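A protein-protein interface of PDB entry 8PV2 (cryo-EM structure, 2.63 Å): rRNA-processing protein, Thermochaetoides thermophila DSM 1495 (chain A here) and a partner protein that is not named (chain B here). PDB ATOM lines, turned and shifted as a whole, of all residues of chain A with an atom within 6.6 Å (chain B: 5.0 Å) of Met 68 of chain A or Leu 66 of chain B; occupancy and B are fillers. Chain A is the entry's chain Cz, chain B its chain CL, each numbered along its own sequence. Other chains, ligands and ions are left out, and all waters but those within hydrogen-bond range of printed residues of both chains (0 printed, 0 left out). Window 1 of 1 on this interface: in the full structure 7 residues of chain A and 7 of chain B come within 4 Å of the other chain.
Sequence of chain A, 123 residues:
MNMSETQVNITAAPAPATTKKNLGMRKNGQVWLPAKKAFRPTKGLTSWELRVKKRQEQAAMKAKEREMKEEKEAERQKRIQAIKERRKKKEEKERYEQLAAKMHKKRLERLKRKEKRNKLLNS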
ATOM      1  N   MET A  61     -17.062 -24.631 -32.502  1.00  0.00           N
ATOM      2  CA  MET A  61     -17.800 -24.524 -31.246  1.00  0.00           C
ATOM      3  C   MET A  61     -18.652 -23.259 -31.208  1.00  0.00           C
ATOM      4  O   MET A  61     -19.796 -23.290 -30.739  1.00  0.00           O
ATOM      5  CB  MET A  61     -16.817 -24.586 -30.069  1.00  0.00           C
ATOM      6  CG  MET A  61     -17.377 -24.335 -28.662  1.00  0.00           C
ATOM      7  SD  MET A  61     -17.619 -22.621 -28.139  1.00  0.00           S
ATOM      8  CE  MET A  61     -15.927 -22.047 -28.075  1.00  0.00           C
ATOM      9  N   ALA A  63     -19.889 -21.638 -33.803  1.00  0.00           N
ATOM     10  CA  ALA A  63     -21.003 -21.830 -34.726  1.00  0.00           C
ATOM     11  C   ALA A  63     -22.108 -22.669 -34.094  1.00  0.00           C
ATOM     12  O   ALA A  63     -23.297 -22.331 -34.192  1.00  0.00           O
ATOM     13  CB  ALA A  63     -20.504 -22.478 -36.016  1.00  0.00           C
ATOM     14  N   LYS A  64     -21.730 -23.757 -33.416  1.00  0.00           N
ATOM     15  CA  LYS A  64     -22.728 -24.617 -32.785  1.00  0.00           C
ATOM     16  C   LYS A  64     -23.466 -23.895 -31.659  1.00  0.00           C
ATOM     17  O   LYS A  64     -24.694 -24.017 -31.529  1.00  0.00           O
ATOM     18  CB  LYS A  64     -22.064 -25.886 -32.263  1.00  0.00           C
ATOM     19  CG  LYS A  64     -22.996 -26.761 -31.472  1.00  0.00           C
ATOM     20  CD  LYS A  64     -22.274 -27.929 -30.862  1.00  0.00           C
ATOM     21  CE  LYS A  64     -23.248 -28.785 -30.099  1.00  0.00           C
ATOM     22  NZ  LYS A  64     -22.585 -29.973 -29.537  1.00  0.00           N
ATOM     23  N   GLU A  65     -22.733 -23.129 -30.845  1.00  0.00           N
ATOM     24  CA  GLU A  65     -23.362 -22.364 -29.774  1.00  0.00           C
ATOM     25  C   GLU A  65     -24.318 -21.318 -30.332  1.00  0.00           C
ATOM     26  O   GLU A  65     -25.395 -21.083 -29.766  1.00  0.00           O
ATOM     27  CB  GLU A  65     -22.293 -21.703 -28.905  1.00  0.00           C
ATOM     28  CG  GLU A  65     -22.851 -20.918 -27.734  1.00  0.00           C
ATOM     29  CD  GLU A  65     -21.802 -20.090 -27.029  1.00  0.00           C
ATOM     30  OE1 GLU A  65     -20.685 -19.958 -27.570  1.00  0.00           O
ATOM     31  OE2 GLU A  65     -22.091 -19.574 -25.929  1.00  0.00           O
ATOM     32  N   ARG A  66     -23.943 -20.684 -31.448  1.00  0.00           N
ATOM     33  CA  ARG A  66     -24.828 -19.720 -32.091  1.00  0.00           C
ATOM     34  C   ARG A  66     -26.109 -20.380 -32.580  1.00  0.00           C
ATOM     35  O   ARG A  66     -27.198 -19.808 -32.439  1.00  0.00           O
ATOM     36  CB  ARG A  66     -24.104 -19.037 -33.250  1.00  0.00           C
ATOM     37  CG  ARG A  66     -23.227 -17.874 -32.835  1.00  0.00           C
ATOM     38  CD  ARG A  66     -22.798 -17.065 -34.044  1.00  0.00           C
ATOM     39  NE  ARG A  66     -22.055 -17.877 -34.999  1.00  0.00           N
ATOM     40  CZ  ARG A  66     -20.797 -17.651 -35.352  1.00  0.00           C
ATOM     41  NH1 ARG A  66     -20.110 -16.637 -34.855  1.00  0.00           N
ATOM     42  NH2 ARG A  66     -20.213 -18.466 -36.226  1.00  0.00           N
ATOM     43  N   GLU A  67     -26.002 -21.584 -33.152  1.00  0.00           N
ATOM     44  CA  GLU A  67     -27.200 -22.295 -33.603  1.00  0.00           C
ATOM     45  C   GLU A  67     -28.125 -22.628 -32.436  1.00  0.00           C
ATOM     46  O   GLU A  67     -29.350 -22.463 -32.533  1.00  0.00           O
ATOM     47  CB  GLU A  67     -26.816 -23.568 -34.358  1.00  0.00           C
ATOM     48  CG  GLU A  67     -25.996 -23.339 -35.615  1.00  0.00           C
ATOM     49  CD  GLU A  67     -26.709 -22.479 -36.639  1.00  0.00           C
ATOM     50  OE1 GLU A  67     -27.943 -22.613 -36.785  1.00  0.00           O
ATOM     51  OE2 GLU A  67     -26.031 -21.665 -37.303  1.00  0.00           O
ATOM     52  N   MET A  68     -27.552 -23.092 -31.319  1.00  0.00           N
ATOM     53  CA  MET A  68     -28.372 -23.426 -30.153  1.00  0.00           C
ATOM     54  C   MET A  68     -29.060 -22.190 -29.579  1.00  0.00           C
ATOM     55  O   MET A  68     -30.248 -22.237 -29.218  1.00  0.00           O
ATOM     56  CB  MET A  68     -27.514 -24.108 -29.089  1.00  0.00           C
ATOM     57  CG  MET A  68     -26.886 -25.414 -29.544  1.00  0.00           C
ATOM     58  SD  MET A  68     -25.954 -26.262 -28.258  1.00  0.00           S
ATOM     59  CE  MET A  68     -27.191 -26.400 -26.975  1.00  0.00           C
ATOM     60  N   LYS A  69     -28.334 -21.070 -29.507  1.00  0.00           N
ATOM     61  CA  LYS A  69     -28.924 -19.830 -29.010  1.00  0.00           C
ATOM     62  C   LYS A  69     -30.030 -19.326 -29.929  1.00  0.00           C
ATOM     63  O   LYS A  69     -31.058 -18.828 -29.454  1.00  0.00           O
ATOM     64  CB  LYS A  69     -27.846 -18.762 -28.840  1.00  0.00           C
ATOM     65  CG  LYS A  69     -26.927 -18.985 -27.655  1.00  0.00           C
ATOM     66  CD  LYS A  69     -25.851 -17.914 -27.595  1.00  0.00           C
ATOM     67  CE  LYS A  69     -25.076 -17.982 -26.292  1.00  0.00           C
ATOM     68  NZ  LYS A  69     -23.995 -16.961 -26.241  1.00  0.00           N
ATOM     69  N   GLU A  70     -29.840 -19.446 -31.248  1.00  0.00           N
ATOM     70  CA  GLU A  70     -30.872 -19.017 -32.188  1.00  0.00           C
ATOM     71  C   GLU A  70     -32.127 -19.871 -32.065  1.00  0.00           C
ATOM     72  O   GLU A  70     -33.249 -19.357 -32.152  1.00  0.00           O
ATOM     73  CB  GLU A  70     -30.335 -19.048 -33.618  1.00  0.00           C
ATOM     74  CG  GLU A  70     -29.390 -17.905 -33.944  1.00  0.00           C
ATOM     75  CD  GLU A  70     -28.569 -18.164 -35.189  1.00  0.00           C
ATOM     76  OE1 GLU A  70     -28.807 -19.193 -35.857  1.00  0.00           O
ATOM     77  OE2 GLU A  70     -27.685 -17.340 -35.502  1.00  0.00           O
ATOM     78  N   GLU A  71     -31.958 -21.181 -31.859  1.00  0.00           N
ATOM     79  CA  GLU A  71     -33.114 -22.058 -31.673  1.00  0.00           C
ATOM     80  C   GLU A  71     -33.894 -21.692 -30.412  1.00  0.00           C
ATOM     81  O   GLU A  71     -35.134 -21.604 -30.431  1.00  0.00           O
ATOM     82  CB  GLU A  71     -32.656 -23.514 -31.624  1.00  0.00           C
ATOM     83  CG  GLU A  71     -33.773 -24.533 -31.780  1.00  0.00           C
ATOM     84  CD  GLU A  71     -34.367 -24.965 -30.454  1.00  0.00           C
ATOM     85  OE1 GLU A  71     -33.643 -24.928 -29.437  1.00  0.00           O
ATOM     86  OE2 GLU A  71     -35.558 -25.340 -30.428  1.00  0.00           O
ATOM     87  N   LYS A  72     -33.177 -21.459 -29.305  1.00  0.00           N
ATOM     88  CA  LYS A  72     -33.844 -21.060 -28.065  1.00  0.00           C
ATOM     89  C   LYS A  72     -34.551 -19.719 -28.216  1.00  0.00           C
ATOM     90  O   LYS A  72     -35.673 -19.539 -27.719  1.00  0.00           O
ATOM     91  CB  LYS A  72     -32.841 -21.002 -26.916  1.00  0.00           C
ATOM     92  CG  LYS A  72     -32.269 -22.346 -26.516  1.00  0.00           C
ATOM     93  CD  LYS A  72     -31.630 -22.269 -25.142  1.00  0.00           C
ATOM     94  CE  LYS A  72     -32.638 -21.837 -24.091  1.00  0.00           C
ATOM     95  NZ  LYS A  72     -32.032 -21.762 -22.736  1.00  0.00           N
ATOM     96  N   GLU A  73     -33.919 -18.772 -28.913  1.00  0.00           N
ATOM     97  CA  GLU A  73     -34.540 -17.471 -29.133  1.00  0.00           C
ATOM     98  C   GLU A  73     -35.791 -17.590 -29.996  1.00  0.00           C
ATOM     99  O   GLU A  73     -36.778 -16.883 -29.766  1.00  0.00           O
ATOM    100  CB  GLU A  73     -33.529 -16.514 -29.767  1.00  0.00           C
ATOM    101  CG  GLU A  73     -34.063 -15.116 -30.040  1.00  0.00           C
ATOM    102  CD  GLU A  73     -34.305 -14.316 -28.774  1.00  0.00           C
ATOM    103  OE1 GLU A  73     -33.699 -14.638 -27.730  1.00  0.00           O
ATOM    104  OE2 GLU A  73     -35.108 -13.360 -28.821  1.00  0.00           O
ATOM    105  N   ILE B  55     -21.232 -20.410 -20.584  1.00  0.00           N
ATOM    106  CA  ILE B  55     -19.981 -21.155 -20.474  1.00  0.00           C
ATOM    107  C   ILE B  55     -18.863 -20.291 -21.048  1.00  0.00           C
ATOM    108  O   ILE B  55     -19.062 -19.669 -22.099  1.00  0.00           O
ATOM    109  CB  ILE B  55     -20.064 -22.495 -21.222  1.00  0.00           C
ATOM    110  CG1 ILE B  55     -21.404 -23.162 -20.952  1.00  0.00           C
ATOM    111  CG2 ILE B  55     -18.939 -23.422 -20.799  1.00  0.00           C
ATOM    112  CD1 ILE B  55     -21.753 -24.187 -21.973  1.00  0.00           C
ATOM    113  N   LYS B  62     -16.087 -27.111 -23.607  1.00  0.00           N
ATOM    114  CA  LYS B  62     -17.383 -26.489 -23.846  1.00  0.00           C
ATOM    115  C   LYS B  62     -18.145 -27.216 -24.946  1.00  0.00           C
ATOM    116  O   LYS B  62     -19.371 -27.354 -24.871  1.00  0.00           O
ATOM    117  CB  LYS B  62     -17.188 -25.012 -24.189  1.00  0.00           C
ATOM    118  CG  LYS B  62     -18.468 -24.253 -24.488  1.00  0.00           C
ATOM    119  CD  LYS B  62     -18.222 -22.765 -24.593  1.00  0.00           C
ATOM    120  CE  LYS B  62     -19.500 -22.027 -24.922  1.00  0.00           C
ATOM    121  NZ  LYS B  62     -19.299 -20.561 -24.973  1.00  0.00           N
ATOM    122  N   GLU B  63     -17.434 -27.722 -25.956  1.00  0.00           N
ATOM    123  CA  GLU B  63     -18.097 -28.408 -27.061  1.00  0.00           C
ATOM    124  C   GLU B  63     -18.725 -29.724 -26.614  1.00  0.00           C
ATOM    125  O   GLU B  63     -19.880 -30.012 -26.951  1.00  0.00           O
ATOM    126  CB  GLU B  63     -17.113 -28.642 -28.205  1.00  0.00           C
ATOM    127  CG  GLU B  63     -17.768 -29.193 -29.456  1.00  0.00           C
ATOM    128  CD  GLU B  63     -17.082 -28.739 -30.726  1.00  0.00           C
ATOM    129  OE1 GLU B  63     -17.784 -28.534 -31.737  1.00  0.00           O
ATOM    130  OE2 GLU B  63     -15.843 -28.583 -30.714  1.00  0.00           O
ATOM    131  N   ARG B  64     -17.993 -30.535 -25.847  1.00  0.00           N
ATOM    132  CA  ARG B  64     -18.588 -31.782 -25.375  1.00  0.00           C
ATOM    133  C   ARG B  64     -19.658 -31.512 -24.326  1.00  0.00           C
ATOM    134  O   ARG B  64     -20.594 -32.304 -24.170  1.00  0.00           O
ATOM    135  CB  ARG B  64     -17.535 -32.744 -24.823  1.00  0.00           C
ATOM    136  CG  ARG B  64     -16.806 -32.267 -23.597  1.00  0.00           C
ATOM    137  CD  ARG B  64     -15.591 -33.127 -23.296  1.00  0.00           C
ATOM    138  NE  ARG B  64     -14.879 -33.568 -24.486  1.00  0.00           N
ATOM    139  CZ  ARG B  64     -13.700 -34.173 -24.458  1.00  0.00           C
ATOM    140  NH1 ARG B  64     -13.081 -34.426 -23.317  1.00  0.00           N
ATOM    141  NH2 ARG B  64     -13.130 -34.537 -25.602  1.00  0.00           N
ATOM    142  N   LEU B  65     -19.557 -30.390 -23.608  1.00  0.00           N
ATOM    143  CA  LEU B  65     -20.618 -30.066 -22.660  1.00  0.00           C
ATOM    144  C   LEU B  65     -21.893 -29.668 -23.403  1.00  0.00           C
ATOM    145  O   LEU B  65     -23.005 -29.989 -22.964  1.00  0.00           O
ATOM    146  CB  LEU B  65     -20.143 -28.962 -21.711  1.00  0.00           C
ATOM    147  CG  LEU B  65     -20.959 -28.536 -20.482  1.00  0.00           C
ATOM    148  CD1 LEU B  65     -20.008 -27.969 -19.450  1.00  0.00           C
ATOM    149  CD2 LEU B  65     -22.064 -27.555 -20.741  1.00  0.00           C
ATOM    150  N   LEU B  66     -21.751 -28.984 -24.544  1.00  0.00           N
ATOM    151  CA  LEU B  66     -22.907 -28.692 -25.391  1.00  0.00           C
ATOM    152  C   LEU B  66     -23.484 -29.963 -26.004  1.00  0.00           C
ATOM    153  O   LEU B  66     -24.706 -30.081 -26.174  1.00  0.00           O
ATOM    154  CB  LEU B  66     -22.521 -27.704 -26.490  1.00  0.00           C
ATOM    155  CG  LEU B  66     -22.174 -26.281 -26.056  1.00  0.00           C
ATOM    156  CD1 LEU B  66     -21.771 -25.439 -27.251  1.00  0.00           C
ATOM    157  CD2 LEU B  66     -23.336 -25.656 -25.320  1.00  0.00           C
ATOM    158  N   GLN B  67     -22.616 -30.918 -26.356  1.00  0.00           N
ATOM    159  CA  GLN B  67     -23.083 -32.229 -26.803  1.00  0.00           C
ATOM    160  C   GLN B  67     -23.905 -32.912 -25.718  1.00  0.00           C
ATOM    161  O   GLN B  67     -24.954 -33.507 -25.994  1.00  0.00           O
ATOM    162  CB  GLN B  67     -21.898 -33.113 -27.192  1.00  0.00           C
ATOM    163  CG  GLN B  67     -21.124 -32.660 -28.409  1.00  0.00           C
ATOM    164  CD  GLN B  67     -19.955 -33.567 -28.725  1.00  0.00           C
ATOM    165  OE1 GLN B  67     -19.672 -34.514 -27.992  1.00  0.00           O
ATOM    166  NE2 GLN B  67     -19.264 -33.280 -29.822  1.00  0.00           N
ATOM    167  N   GLN B  68     -23.436 -32.828 -24.472  1.00  0.00           N
ATOM    168  CA  GLN B  68     -24.163 -33.393 -23.342  1.00  0.00           C
ATOM    169  C   GLN B  68     -25.514 -32.713 -23.155  1.00  0.00           C
ATOM    170  O   GLN B  68     -26.515 -33.373 -22.861  1.00  0.00           O
ATOM    171  CB  GLN B  68     -23.317 -33.269 -22.075  1.00  0.00           C
ATOM    172  CG  GLN B  68     -23.934 -33.903 -20.847  1.00  0.00           C
ATOM    173  CD  GLN B  68     -23.036 -33.804 -19.634  1.00  0.00           C
ATOM    174  OE1 GLN B  68     -21.952 -33.225 -19.696  1.00  0.00           O
ATOM    175  NE2 GLN B  68     -23.482 -34.373 -18.520  1.00  0.00           N
ATOM    176  N   ILE B  69     -25.557 -31.387 -23.324  1.00  0.00           N
ATOM    177  CA  ILE B  69     -26.814 -30.651 -23.180  1.00  0.00           C
ATOM    178  C   ILE B  69     -27.817 -31.066 -24.253  1.00  0.00           C
ATOM    179  O   ILE B  69     -28.996 -31.309 -23.958  1.00  0.00           O
ATOM    180  CB  ILE B  69     -26.554 -29.133 -23.205  1.00  0.00           C
ATOM    181  CG1 ILE B  69     -25.886 -28.682 -21.908  1.00  0.00           C
ATOM    182  CG2 ILE B  69     -27.840 -28.359 -23.424  1.00  0.00           C
ATOM    183  CD1 ILE B  69     -25.515 -27.224 -21.908  1.00  0.00           C
ATOM    184  N   GLU B  70     -27.369 -31.163 -25.509  1.00  0.00           N
ATOM    185  CA  GLU B  70     -28.272 -31.580 -26.582  1.00  0.00           C
ATOM    186  C   GLU B  70     -28.751 -33.013 -26.383  1.00  0.00           C
ATOM    187  O   GLU B  70     -29.926 -33.323 -26.617  1.00  0.00           O
ATOM    188  CB  GLU B  70     -27.601 -31.428 -27.945  1.00  0.00           C
ATOM    189  CG  GLU B  70     -27.331 -29.999 -28.358  1.00  0.00           C
ATOM    190  CD  GLU B  70     -26.654 -29.913 -29.709  1.00  0.00           C
ATOM    191  OE1 GLU B  70     -26.285 -30.973 -30.257  1.00  0.00           O
ATOM    192  OE2 GLU B  70     -26.513 -28.791 -30.237  1.00  0.00           O
ATOM    193  N   GLU B  71     -27.854 -33.900 -25.945  1.00  0.00           N
ATOM    194  CA  GLU B  71     -28.237 -35.285 -25.686  1.00  0.00           C
ATOM    195  C   GLU B  71     -29.252 -35.372 -24.552  1.00  0.00           C
ATOM    196  O   GLU B  71     -30.204 -36.158 -24.615  1.00  0.00           O
ATOM    197  CB  GLU B  71     -26.991 -36.114 -25.373  1.00  0.00           C
ATOM    198  CG  GLU B  71     -27.271 -37.502 -24.828  1.00  0.00           C
ATOM    199  CD  GLU B  71     -26.034 -38.160 -24.256  1.00  0.00           C
ATOM    200  OE1 GLU B  71     -24.985 -37.489 -24.180  1.00  0.00           O
ATOM    201  OE2 GLU B  71     -26.113 -39.350 -23.884  1.00  0.00           O
ATOM    202  N   ARG B  73     -31.392 -33.007 -23.736  1.00  0.00           N
ATOM    203  CA  ARG B  73     -32.663 -32.517 -24.273  1.00  0.00           C
ATOM    204  C   ARG B  73     -33.372 -33.581 -25.103  1.00  0.00           C
ATOM    205  O   ARG B  73     -34.594 -33.745 -24.993  1.00  0.00           O
ATOM    206  CB  ARG B  73     -32.452 -31.260 -25.112  1.00  0.00           C
ATOM    207  CG  ARG B  73     -32.016 -30.040 -24.338  1.00  0.00           C
ATOM    208  CD  ARG B  73     -31.842 -28.865 -25.280  1.00  0.00           C
ATOM    209  NE  ARG B  73     -31.403 -27.665 -24.582  1.00  0.00           N
ATOM    210  CZ  ARG B  73     -31.122 -26.515 -25.177  1.00  0.00           C
ATOM    211  NH1 ARG B  73     -31.187 -26.382 -26.490  1.00  0.00           N
ATOM    212  NH2 ARG B  73     -30.773 -25.470 -24.433  1.00  0.00           N
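NZ of Lys 64 of chain A is in salt-bridge range of OE1 of Glu 70 of chain B, at 3.9 Å. The side-chain amino group (NZ) of Lys 62 of chain B lies within salt-bridge range of the side-chain carboxylate (OE1) of Glu 65 of chain A (3.0 Å). The side-chain amino group of Lys 64 of chain A lies close to the backbone NH of Gln 67 of chain B, 3.3 Å away. The side-chain carboxylate (OE2) of Glu 70 of chain B sits close to the side-chain sulfur (SD) of Met 68 of chain A, 3.3 Å away.
OE2 of Glu 65 of chain A lies within salt-bridge range of NZ of Lys 69 of chain A (3.2 Å). O of Ile 55 of chain B is in hydrogen-bond range of NZ of Lys 62 of chain B (3.0 Å).
Among the printed residues, merely in contact across the chains: Met 61 of chain A with Lys 62 of chain B (3.6 Å), Lys 64 of chain A with Glu 63 of chain B (3.7 Å), Lys 64 of chain A with Leu 66 of chain B (3.6 Å), Met 68 of chain A with Leu 66 of chain B (3.98 Å) and Lys 72 of chain A with Arg 73 of chain B (3.4 Å).
Printed residues of chain B within 4 Å of Lys 64 of chain A: Glu 63, Leu 66, Gln 67 and Glu 70. Of the printed residues of chain B, Met 68 of chain A touches Leu 66 and Glu 70. Of the printed residues of chain A, Lys 62 of chain B touches Met 61 and Glu 65. Arg 64 of chain B touches none of the printed residues of chain A. Printed residues of chain A within 4 Å of Leu 66 of chain B: Lys 64 and Met 68. Printed residues of chain A within 4 Å of Gln 67 of chain B: Lys 64 (3.3 Å). Glu 71 of chain B touches none of the printed residues of chain A. The nearest printed residue of chain B that does not touch Met 68 of chain A is Arg 73 of chain B (4.03 Å). The nearest printed residue of chain A that does not touch Leu 66 of chain B is Glu 65 of chain A (4.1 Å). The nearest printed residue of chain A that does not touch Lys 62 of chain B is Lys 69 of chain A (6.1 Å).
Hydrophobic or aromatic side chains of chain B within 4 Å of the printed part of chain A: Leu 66. Among the printed residues, Asp or Glu carboxylates within 4 Å of a Lys or Arg side-chain nitrogen of the other chain: Lys 64 of chain A with Glu 70 of chain B (3.9 Å) and Glu 65 of chain A with Lys 62 of chain B (3.0 Å).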
